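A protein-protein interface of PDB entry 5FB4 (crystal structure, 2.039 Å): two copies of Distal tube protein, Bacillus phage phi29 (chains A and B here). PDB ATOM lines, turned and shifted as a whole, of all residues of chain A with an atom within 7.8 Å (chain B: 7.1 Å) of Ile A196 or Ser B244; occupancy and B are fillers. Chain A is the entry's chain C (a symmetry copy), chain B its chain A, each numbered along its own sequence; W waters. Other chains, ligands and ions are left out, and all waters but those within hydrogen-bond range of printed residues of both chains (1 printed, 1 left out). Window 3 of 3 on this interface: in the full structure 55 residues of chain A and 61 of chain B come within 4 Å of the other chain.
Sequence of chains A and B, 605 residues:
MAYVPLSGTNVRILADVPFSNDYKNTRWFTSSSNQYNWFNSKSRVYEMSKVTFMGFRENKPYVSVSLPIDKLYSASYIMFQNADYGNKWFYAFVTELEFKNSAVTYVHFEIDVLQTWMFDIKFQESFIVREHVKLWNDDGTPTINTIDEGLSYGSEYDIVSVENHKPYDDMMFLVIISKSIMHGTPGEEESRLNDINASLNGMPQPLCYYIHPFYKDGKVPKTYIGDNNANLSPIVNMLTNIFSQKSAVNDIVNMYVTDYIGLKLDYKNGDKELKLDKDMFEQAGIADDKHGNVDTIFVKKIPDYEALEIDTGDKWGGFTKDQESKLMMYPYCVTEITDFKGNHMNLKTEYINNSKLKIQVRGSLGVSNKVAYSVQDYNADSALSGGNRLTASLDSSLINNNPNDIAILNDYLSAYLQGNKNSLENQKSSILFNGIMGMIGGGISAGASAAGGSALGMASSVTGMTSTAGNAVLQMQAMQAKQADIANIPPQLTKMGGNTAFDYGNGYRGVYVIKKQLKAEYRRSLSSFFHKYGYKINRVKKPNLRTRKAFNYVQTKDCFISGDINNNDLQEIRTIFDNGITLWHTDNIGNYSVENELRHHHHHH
Water W1 bridges OG of Ser B244 (2.9 Å) and N of Ile A196 (2.9 Å).
No position is printed for both chains.
O of Thr B240 lies within hydrogen-bond range of OG of Ser B244, at 2.8 Å.
ND1 of His B291 lies within hydrogen-bond range of O of Ser B244.
The backbone NH (N) of Lys A179 lies within hydrogen-bond range of the backbone carbonyl oxygen (O) of Asp A251.
The backbone NH (N) of Ser A199 is in hydrogen-bond range of the backbone carbonyl oxygen (O) of Gln A205, at 2.7 Å.
N of Leu A207 sits close to NE2 of Gln A205.
Lys A179 touches Leu B409.
O of Ile A196 touches CG2 of Thr B240 (3.6 Å).
Ile A196 touches Ser B244.
Leu B409 touches Ile A196.
Thr B240 touches Asn A197.
CB of Leu B239 touches CB of Ala A198, at 3.6 Å.
CD1 of Leu B239 touches N of Gln A205, 3.7 Å away.
Phe B243 touches Pro A206.
Pro A206 touches Leu B409 (O to CD1, 3.5 Å).
Leu A207 touches Leu B409.
Of the 17 printed residues of chain B, 5 touch a printed residue of chain A.
Printed residues of chain B that touch a printed residue of chain A: Leu B239, Thr B240, Phe B243, Ser B244 and Leu B409.
Hydrophobic or aromatic side chains of chain A within 4 Å of the printed part of chain B: Ile A196, Ala A198, Pro A206 and Leu A207.
Among the printed residues, no Asp or Glu carboxylate lies within 4 Å of a Lys or Arg side-chain nitrogen of the other chain.
Ile A196 touches three residues of chain B.
Ser B244 touches just one residue of chain A: Ile A196.
Printed residues of chain B within 4 Å of Lys A179: Leu B409.
Printed residues of chain B within 4 Å of Leu A207: Leu B409.
Arg A192 touches none of the printed residues of chain B.
Asn B241 touches none of the printed residues of chain A.
The nearest printed residue of chain B that does not touch Ala A198 is Met B238 (6.2 Å).
N of Ala A198 sits at hydrogen-bond distance from OG1 of Thr B240, at 3.0 Å.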
ATOM      1  N   SER A 178     -12.607  32.202  14.984  1.00  0.00           N
ATOM      2  CA  SER A 178     -14.008  32.041  15.346  1.00  0.00           C
ATOM      3  C   SER A 178     -14.174  31.195  16.599  1.00  0.00           C
ATOM      4  O   SER A 178     -13.252  30.488  17.022  1.00  0.00           O
ATOM      5  CB  SER A 178     -14.811  31.441  14.179  1.00  0.00           C
ATOM      6  OG  SER A 178     -14.416  30.119  13.904  1.00  0.00           O
ATOM      7  N   LYS A 179     -15.363  31.286  17.190  1.00  0.00           N
ATOM      8  CA  LYS A 179     -15.679  30.597  18.436  1.00  0.00           C
ATOM      9  C   LYS A 179     -15.976  29.127  18.189  1.00  0.00           C
ATOM     10  O   LYS A 179     -15.904  28.306  19.105  1.00  0.00           O
ATOM     11  CB  LYS A 179     -16.888  31.244  19.122  1.00  0.00           C
ATOM     12  CG  LYS A 179     -16.680  32.674  19.568  1.00  0.00           C
ATOM     13  CD  LYS A 179     -17.776  33.581  19.009  1.00  0.00           C
ATOM     14  CE  LYS A 179     -19.166  33.135  19.427  1.00  0.00           C
ATOM     15  NZ  LYS A 179     -19.554  33.656  20.765  1.00  0.00           N
ATOM     16  N   SER A 180     -16.300  28.793  16.947  1.00  0.00           N
ATOM     17  CA  SER A 180     -16.639  27.412  16.620  1.00  0.00           C
ATOM     18  C   SER A 180     -16.311  27.070  15.175  1.00  0.00           C
ATOM     19  O   SER A 180     -15.987  27.942  14.371  1.00  0.00           O
ATOM     20  CB  SER A 180     -18.120  27.144  16.896  1.00  0.00           C
ATOM     21  OG  SER A 180     -18.939  27.950  16.069  1.00  0.00           O
ATOM     22  N   ILE A 181     -16.403  25.787  14.852  1.00  0.00           N
ATOM     23  CA  ILE A 181     -16.068  25.317  13.520  1.00  0.00           C
ATOM     24  C   ILE A 181     -17.068  25.832  12.482  1.00  0.00           C
ATOM     25  O   ILE A 181     -18.278  25.714  12.659  1.00  0.00           O
ATOM     26  CB  ILE A 181     -15.983  23.782  13.503  1.00  0.00           C
ATOM     27  CG1 ILE A 181     -14.632  23.356  14.114  1.00  0.00           C
ATOM     28  CG2 ILE A 181     -16.096  23.261  12.089  1.00  0.00           C
ATOM     29  CD1 ILE A 181     -14.444  21.856  14.197  1.00  0.00           C
ATOM     30  N   ARG A 192     -19.298  19.028  11.421  1.00  0.00           N
ATOM     31  CA  ARG A 192     -18.819  19.549  12.699  1.00  0.00           C
ATOM     32  C   ARG A 192     -19.203  21.013  12.871  1.00  0.00           C
ATOM     33  O   ARG A 192     -18.670  21.690  13.753  1.00  0.00           O
ATOM     34  CB  ARG A 192     -17.295  19.405  12.835  1.00  0.00           C
ATOM     35  CG  ARG A 192     -16.817  17.958  12.990  1.00  0.00           C
ATOM     36  CD  ARG A 192     -15.288  17.906  13.030  1.00  0.00           C
ATOM     37  NE  ARG A 192     -14.670  18.224  11.743  1.00  0.00           N
ATOM     38  CZ  ARG A 192     -13.426  18.686  11.609  1.00  0.00           C
ATOM     39  NH1 ARG A 192     -12.674  18.901  12.684  1.00  0.00           N
ATOM     40  NH2 ARG A 192     -12.937  18.945  10.403  1.00  0.00           N
ATOM     41  N   LEU A 193     -20.107  21.503  12.017  1.00  0.00           N
ATOM     42  CA  LEU A 193     -20.487  22.917  12.031  1.00  0.00           C
ATOM     43  C   LEU A 193     -20.993  23.342  13.401  1.00  0.00           C
ATOM     44  O   LEU A 193     -21.874  22.699  13.973  1.00  0.00           O
ATOM     45  CB  LEU A 193     -21.567  23.209  10.979  1.00  0.00           C
ATOM     46  CG  LEU A 193     -21.142  23.186   9.515  1.00  0.00           C
ATOM     47  CD1 LEU A 193     -22.345  23.495   8.615  1.00  0.00           C
ATOM     48  CD2 LEU A 193     -19.998  24.175   9.276  1.00  0.00           C
ATOM     49  N   ASN A 194     -20.441  24.444  13.895  1.00  0.00           N
ATOM     50  CA  ASN A 194     -20.796  25.023  15.191  1.00  0.00           C
ATOM     51  C   ASN A 194     -20.259  24.243  16.389  1.00  0.00           C
ATOM     52  O   ASN A 194     -20.577  24.572  17.526  1.00  0.00           O
ATOM     53  CB  ASN A 194     -22.313  25.187  15.319  1.00  0.00           C
ATOM     54  CG  ASN A 194     -22.886  26.083  14.248  1.00  0.00           C
ATOM     55  OD1 ASN A 194     -22.360  27.162  13.978  1.00  0.00           O
ATOM     56  ND2 ASN A 194     -23.978  25.650  13.641  1.00  0.00           N
ATOM     57  N   ASP A 195     -19.474  23.196  16.151  1.00  0.00           N
ATOM     58  CA  ASP A 195     -18.787  22.542  17.264  1.00  0.00           C
ATOM     59  C   ASP A 195     -17.698  23.444  17.850  1.00  0.00           C
ATOM     60  O   ASP A 195     -16.951  24.094  17.107  1.00  0.00           O
ATOM     61  CB  ASP A 195     -18.142  21.222  16.834  1.00  0.00           C
ATOM     62  CG  ASP A 195     -19.151  20.138  16.520  1.00  0.00           C
ATOM     63  OD1 ASP A 195     -20.372  20.351  16.705  1.00  0.00           O
ATOM     64  OD2 ASP A 195     -18.700  19.054  16.092  1.00  0.00           O
ATOM     65  N   ILE A 196     -17.595  23.459  19.178  1.00  0.00           N
ATOM     66  CA  ILE A 196     -16.397  23.995  19.829  1.00  0.00           C
ATOM     67  C   ILE A 196     -15.230  23.092  19.455  1.00  0.00           C
ATOM     68  O   ILE A 196     -15.391  21.876  19.383  1.00  0.00           O
ATOM     69  CB  ILE A 196     -16.526  24.033  21.373  1.00  0.00           C
ATOM     70  CG1 ILE A 196     -17.763  24.827  21.797  1.00  0.00           C
ATOM     71  CG2 ILE A 196     -15.239  24.586  22.010  1.00  0.00           C
ATOM     72  CD1 ILE A 196     -17.746  26.256  21.324  1.00  0.00           C
ATOM     73  N   ASN A 197     -14.057  23.662  19.222  1.00  0.00           N
ATOM     74  CA  ASN A 197     -12.892  22.835  18.934  1.00  0.00           C
ATOM     75  C   ASN A 197     -11.633  23.458  19.523  1.00  0.00           C
ATOM     76  O   ASN A 197     -11.023  24.341  18.921  1.00  0.00           O
ATOM     77  CB  ASN A 197     -12.721  22.635  17.421  1.00  0.00           C
ATOM     78  CG  ASN A 197     -11.581  21.681  17.084  1.00  0.00           C
ATOM     79  OD1 ASN A 197     -10.453  22.102  16.816  1.00  0.00           O
ATOM     80  ND2 ASN A 197     -11.872  20.395  17.097  1.00  0.00           N
ATOM     81  N   ALA A 198     -11.241  23.002  20.705  1.00  0.00           N
ATOM     82  CA  ALA A 198      -9.992  23.478  21.288  1.00  0.00           C
ATOM     83  C   ALA A 198      -8.828  22.764  20.599  1.00  0.00           C
ATOM     84  O   ALA A 198      -9.002  21.685  20.023  1.00  0.00           O
ATOM     85  CB  ALA A 198      -9.974  23.237  22.802  1.00  0.00           C
ATOM     86  N   SER A 199      -7.645  23.363  20.653  1.00  0.00           N
ATOM     87  CA  SER A 199      -6.488  22.751  20.030  1.00  0.00           C
ATOM     88  C   SER A 199      -5.185  23.299  20.572  1.00  0.00           C
ATOM     89  O   SER A 199      -5.147  24.386  21.161  1.00  0.00           O
ATOM     90  CB  SER A 199      -6.527  22.964  18.513  1.00  0.00           C
ATOM     91  OG  SER A 199      -6.436  24.342  18.200  1.00  0.00           O
ATOM     92  N   GLN A 205      -5.662  25.773  23.770  1.00  0.00           N
ATOM     93  CA  GLN A 205      -6.423  26.988  23.542  1.00  0.00           C
ATOM     94  C   GLN A 205      -7.761  26.634  22.875  1.00  0.00           C
ATOM     95  O   GLN A 205      -7.816  25.672  22.120  1.00  0.00           O
ATOM     96  CB  GLN A 205      -5.559  27.913  22.688  1.00  0.00           C
ATOM     97  CG  GLN A 205      -6.239  29.008  22.002  1.00  0.00           C
ATOM     98  CD  GLN A 205      -6.909  28.584  20.721  1.00  0.00           C
ATOM     99  OE1 GLN A 205      -6.641  27.517  20.143  1.00  0.00           O
ATOM    100  NE2 GLN A 205      -7.768  29.432  20.252  1.00  0.00           N
ATOM    101  N   PRO A 206      -8.834  27.409  23.150  1.00  0.00           N
ATOM    102  CA  PRO A 206     -10.217  27.004  22.820  1.00  0.00           C
ATOM    103  C   PRO A 206     -10.828  27.548  21.510  1.00  0.00           C
ATOM    104  O   PRO A 206     -11.963  27.186  21.207  1.00  0.00           O
ATOM    105  CB  PRO A 206     -11.009  27.537  24.015  1.00  0.00           C
ATOM    106  CG  PRO A 206     -10.297  28.844  24.332  1.00  0.00           C
ATOM    107  CD  PRO A 206      -8.812  28.591  24.032  1.00  0.00           C
ATOM    108  N   LEU A 207     -10.128  28.399  20.771  1.00  0.00           N
ATOM    109  CA  LEU A 207     -10.702  29.023  19.568  1.00  0.00           C
ATOM    110  C   LEU A 207     -10.315  28.282  18.280  1.00  0.00           C
ATOM    111  O   LEU A 207      -9.319  27.547  18.244  1.00  0.00           O
ATOM    112  CB  LEU A 207     -10.260  30.499  19.464  1.00  0.00           C
ATOM    113  CG  LEU A 207     -10.718  31.393  20.621  1.00  0.00           C
ATOM    114  CD1 LEU A 207     -10.122  32.789  20.529  1.00  0.00           C
ATOM    115  CD2 LEU A 207     -12.227  31.456  20.623  1.00  0.00           C
ATOM    116  N   CYS A 208     -11.092  28.512  17.226  1.00  0.00           N
ATOM    117  CA  CYS A 208     -10.829  27.956  15.902  1.00  0.00           C
ATOM    118  C   CYS A 208     -10.091  28.957  15.022  1.00  0.00           C
ATOM    119  O   CYS A 208     -10.546  30.085  14.845  1.00  0.00           O
ATOM    120  CB  CYS A 208     -12.139  27.561  15.202  1.00  0.00           C
ATOM    121  SG  CYS A 208     -12.967  26.172  15.947  1.00  0.00           S
ATOM    122  N   ASP A 251     -20.047  34.243  14.199  1.00  0.00           N
ATOM    123  CA  ASP A 251     -19.186  33.403  15.028  1.00  0.00           C
ATOM    124  C   ASP A 251     -17.730  33.896  15.037  1.00  0.00           C
ATOM    125  O   ASP A 251     -16.903  33.430  15.829  1.00  0.00           O
ATOM    126  CB  ASP A 251     -19.250  31.961  14.520  1.00  0.00           C
ATOM    127  CG  ASP A 251     -19.082  30.941  15.630  1.00  0.00           C
ATOM    128  OD1 ASP A 251     -20.000  30.817  16.476  1.00  0.00           O
ATOM    129  OD2 ASP A 251     -18.036  30.256  15.643  1.00  0.00           O
ATOM    130  N   MET B 238     -10.571  18.751  27.475  1.00  0.00           N
ATOM    131  CA  MET B 238     -11.251  19.382  28.583  1.00  0.00           C
ATOM    132  C   MET B 238     -11.774  20.766  28.220  1.00  0.00           C
ATOM    133  O   MET B 238     -12.904  21.132  28.567  1.00  0.00           O
ATOM    134  CB  MET B 238     -10.328  19.472  29.773  1.00  0.00           C
ATOM    135  CG  MET B 238     -11.050  19.978  30.972  1.00  0.00           C
ATOM    136  SD  MET B 238      -9.899  20.455  32.247  1.00  0.00           S
ATOM    137  CE  MET B 238     -10.964  21.402  33.329  1.00  0.00           C
ATOM    138  N   LEU B 239     -10.950  21.532  27.512  1.00  0.00           N
ATOM    139  CA  LEU B 239     -11.371  22.843  27.044  1.00  0.00           C
ATOM    140  C   LEU B 239     -12.563  22.738  26.103  1.00  0.00           C
ATOM    141  O   LEU B 239     -13.518  23.490  26.227  1.00  0.00           O
ATOM    142  CB  LEU B 239     -10.215  23.577  26.356  1.00  0.00           C
ATOM    143  CG  LEU B 239      -9.099  24.107  27.259  1.00  0.00           C
ATOM    144  CD1 LEU B 239      -7.970  24.665  26.416  1.00  0.00           C
ATOM    145  CD2 LEU B 239      -9.643  25.179  28.207  1.00  0.00           C
ATOM    146  N   THR B 240     -12.506  21.805  25.164  1.00  0.00           N
ATOM    147  CA  THR B 240     -13.622  21.600  24.252  1.00  0.00           C
ATOM    148  C   THR B 240     -14.897  21.282  25.030  1.00  0.00           C
ATOM    149  O   THR B 240     -15.959  21.859  24.780  1.00  0.00           O
ATOM    150  CB  THR B 240     -13.357  20.450  23.267  1.00  0.00           C
ATOM    151  OG1 THR B 240     -12.265  20.788  22.406  1.00  0.00           O
ATOM    152  CG2 THR B 240     -14.610  20.151  22.416  1.00  0.00           C
ATOM    153  N   ASN B 241     -14.783  20.366  25.983  1.00  0.00           N
ATOM    154  CA  ASN B 241     -15.961  19.873  26.690  1.00  0.00           C
ATOM    155  C   ASN B 241     -16.529  20.888  27.677  1.00  0.00           C
ATOM    156  O   ASN B 241     -17.743  21.047  27.771  1.00  0.00           O
ATOM    157  CB  ASN B 241     -15.632  18.558  27.393  1.00  0.00           C
ATOM    158  CG  ASN B 241     -15.368  17.432  26.403  1.00  0.00           C
ATOM    159  OD1 ASN B 241     -15.793  17.494  25.251  1.00  0.00           O
ATOM    160  ND2 ASN B 241     -14.651  16.412  26.842  1.00  0.00           N
ATOM    161  N   ILE B 242     -15.660  21.574  28.407  1.00  0.00           N
ATOM    162  CA  ILE B 242     -16.115  22.563  29.377  1.00  0.00           C
ATOM    163  C   ILE B 242     -16.895  23.683  28.673  1.00  0.00           C
ATOM    164  O   ILE B 242     -17.939  24.117  29.160  1.00  0.00           O
ATOM    165  CB  ILE B 242     -14.936  23.160  30.190  1.00  0.00           C
ATOM    166  CG1 ILE B 242     -15.455  23.905  31.418  1.00  0.00           C
ATOM    167  CG2 ILE B 242     -14.077  24.070  29.333  1.00  0.00           C
ATOM    168  CD1 ILE B 242     -15.908  22.994  32.525  1.00  0.00           C
ATOM    169  N   PHE B 243     -16.403  24.138  27.521  1.00  0.00           N
ATOM    170  CA  PHE B 243     -17.063  25.221  26.793  1.00  0.00           C
ATOM    171  C   PHE B 243     -18.283  24.744  26.015  1.00  0.00           C
ATOM    172  O   PHE B 243     -19.082  25.549  25.570  1.00  0.00           O
ATOM    173  CB  PHE B 243     -16.078  25.915  25.853  1.00  0.00           C
ATOM    174  CG  PHE B 243     -15.173  26.888  26.556  1.00  0.00           C
ATOM    175  CD1 PHE B 243     -15.689  27.768  27.496  1.00  0.00           C
ATOM    176  CD2 PHE B 243     -13.809  26.895  26.318  1.00  0.00           C
ATOM    177  CE1 PHE B 243     -14.862  28.663  28.158  1.00  0.00           C
ATOM    178  CE2 PHE B 243     -12.972  27.792  26.983  1.00  0.00           C
ATOM    179  CZ  PHE B 243     -13.501  28.675  27.898  1.00  0.00           C
ATOM    180  N   SER B 244     -18.432  23.434  25.867  1.00  0.00           N
ATOM    181  CA  SER B 244     -19.613  22.874  25.229  1.00  0.00           C
ATOM    182  C   SER B 244     -20.800  22.793  26.195  1.00  0.00           C
ATOM    183  O   SER B 244     -21.947  22.741  25.769  1.00  0.00           O
ATOM    184  CB  SER B 244     -19.303  21.492  24.665  1.00  0.00           C
ATOM    185  OG  SER B 244     -18.439  21.585  23.548  1.00  0.00           O
ATOM    186  N   GLN B 245     -20.510  22.778  27.492  1.00  0.00           N
ATOM    187  CA  GLN B 245     -21.536  22.686  28.528  1.00  0.00           C
ATOM    188  C   GLN B 245     -22.039  24.071  28.946  1.00  0.00           C
ATOM    189  O   GLN B 245     -21.348  24.778  29.676  1.00  0.00           O
ATOM    190  CB  GLN B 245     -20.969  21.948  29.748  1.00  0.00           C
ATOM    191  CG  GLN B 245     -20.501  20.516  29.454  1.00  0.00           C
ATOM    192  CD  GLN B 245     -20.055  19.770  30.704  1.00  0.00           C
ATOM    193  OE1 GLN B 245     -20.599  19.972  31.786  1.00  0.00           O
ATOM    194  NE2 GLN B 245     -19.058  18.901  30.555  1.00  0.00           N
ATOM    195  N   LYS B 246     -23.237  24.454  28.509  1.00  0.00           N
ATOM    196  CA  LYS B 246     -23.768  25.793  28.811  1.00  0.00           C
ATOM    197  C   LYS B 246     -23.912  26.171  30.288  1.00  0.00           C
ATOM    198  O   LYS B 246     -23.647  27.326  30.641  1.00  0.00           O
ATOM    199  CB  LYS B 246     -25.104  26.005  28.096  1.00  0.00           C
ATOM    200  CG  LYS B 246     -25.068  25.582  26.642  1.00  0.00           C
ATOM    201  CD  LYS B 246     -24.026  26.436  25.900  1.00  0.00           C
ATOM    202  CE  LYS B 246     -23.987  26.149  24.403  1.00  0.00           C
ATOM    203  NZ  LYS B 246     -25.299  26.420  23.737  1.00  0.00           N
ATOM    204  N   SER B 247     -24.375  25.256  31.137  1.00  0.00           N
ATOM    205  CA  SER B 247     -24.421  25.550  32.567  1.00  0.00           C
ATOM    206  C   SER B 247     -23.031  25.946  33.080  1.00  0.00           C
ATOM    207  O   SER B 247     -22.885  26.964  33.753  1.00  0.00           O
ATOM    208  CB  SER B 247     -24.982  24.365  33.363  1.00  0.00           C
ATOM    209  OG  SER B 247     -24.324  23.159  33.034  1.00  0.00           O
ATOM    210  N   ALA B 248     -22.010  25.157  32.746  1.00  0.00           N
ATOM    211  CA  ALA B 248     -20.645  25.476  33.174  1.00  0.00           C
ATOM    212  C   ALA B 248     -20.208  26.847  32.655  1.00  0.00           C
ATOM    213  O   ALA B 248     -19.806  27.716  33.431  1.00  0.00           O
ATOM    214  CB  ALA B 248     -19.657  24.400  32.711  1.00  0.00           C
ATOM    215  N   VAL B 249     -20.304  27.048  31.345  1.00  0.00           N
ATOM    216  CA  VAL B 249     -19.755  28.251  30.741  1.00  0.00           C
ATOM    217  C   VAL B 249     -20.424  29.539  31.241  1.00  0.00           C
ATOM    218  O   VAL B 249     -19.745  30.534  31.478  1.00  0.00           O
ATOM    219  CB  VAL B 249     -19.859  28.199  29.201  1.00  0.00           C
ATOM    220  CG1 VAL B 249     -21.230  27.732  28.766  1.00  0.00           C
ATOM    221  CG2 VAL B 249     -19.552  29.565  28.615  1.00  0.00           C
ATOM    222  N   ASP B 288     -22.719  17.188  31.801  1.00  0.00           N
ATOM    223  CA  ASP B 288     -24.096  17.531  31.456  1.00  0.00           C
ATOM    224  C   ASP B 288     -24.802  16.386  30.734  1.00  0.00           C
ATOM    225  O   ASP B 288     -25.934  16.541  30.259  1.00  0.00           O
ATOM    226  CB  ASP B 288     -24.130  18.793  30.586  1.00  0.00           C
ATOM    227  CG  ASP B 288     -23.518  18.577  29.208  1.00  0.00           C
ATOM    228  OD1 ASP B 288     -22.847  17.542  28.996  1.00  0.00           O
ATOM    229  OD2 ASP B 288     -23.717  19.441  28.329  1.00  0.00           O
ATOM    230  N   LYS B 290     -24.371  15.216  27.932  1.00  0.00           N
ATOM    231  CA  LYS B 290     -24.537  15.454  26.496  1.00  0.00           C
ATOM    232  C   LYS B 290     -23.206  15.627  25.743  1.00  0.00           C
ATOM    233  O   LYS B 290     -23.017  15.037  24.680  1.00  0.00           O
ATOM    234  CB  LYS B 290     -25.413  16.697  26.276  1.00  0.00           C
ATOM    235  CG  LYS B 290     -25.617  17.137  24.813  1.00  0.00           C
ATOM    236  CD  LYS B 290     -26.397  16.121  23.982  1.00  0.00           C
ATOM    237  CE  LYS B 290     -26.835  16.723  22.640  1.00  0.00           C
ATOM    238  NZ  LYS B 290     -27.577  15.762  21.755  1.00  0.00           N
ATOM    239  N   HIS B 291     -22.299  16.434  26.299  1.00  0.00           N
ATOM    240  CA  HIS B 291     -21.019  16.756  25.648  1.00  0.00           C
ATOM    241  C   HIS B 291     -19.719  16.141  26.172  1.00  0.00           C
ATOM    242  O   HIS B 291     -18.636  16.630  25.846  1.00  0.00           O
ATOM    243  CB  HIS B 291     -20.823  18.271  25.646  1.00  0.00           C
ATOM    244  CG  HIS B 291     -21.873  19.013  24.883  1.00  0.00           C
ATOM    245  ND1 HIS B 291     -22.899  19.688  25.497  1.00  0.00           N
ATOM    246  CD2 HIS B 291     -22.055  19.164  23.549  1.00  0.00           C
ATOM    247  CE1 HIS B 291     -23.675  20.236  24.572  1.00  0.00           C
ATOM    248  NE2 HIS B 291     -23.183  19.933  23.386  1.00  0.00           N
ATOM    249  N   GLY B 292     -19.793  15.098  26.978  1.00  0.00           N
ATOM    250  CA  GLY B 292     -18.568  14.488  27.478  1.00  0.00           C
ATOM    251  C   GLY B 292     -18.041  15.136  28.740  1.00  0.00           C
ATOM    252  O   GLY B 292     -17.919  16.367  28.856  1.00  0.00           O
ATOM    253  N   LEU B 409     -15.414  31.172  25.971  1.00  0.00           N
ATOM    254  CA  LEU B 409     -16.416  31.040  24.907  1.00  0.00           C
ATOM    255  C   LEU B 409     -17.846  31.101  25.440  1.00  0.00           C
ATOM    256  O   LEU B 409     -18.479  30.065  25.622  1.00  0.00           O
ATOM    257  CB  LEU B 409     -16.219  29.730  24.139  1.00  0.00           C
ATOM    258  CG  LEU B 409     -14.880  29.575  23.421  1.00  0.00           C
ATOM    259  CD1 LEU B 409     -14.956  28.484  22.369  1.00  0.00           C
ATOM    260  CD2 LEU B 409     -14.447  30.896  22.809  1.00  0.00           C
HETATM  261  O   HOH W   1     -19.203  21.696  20.783  1.00  0.00           O
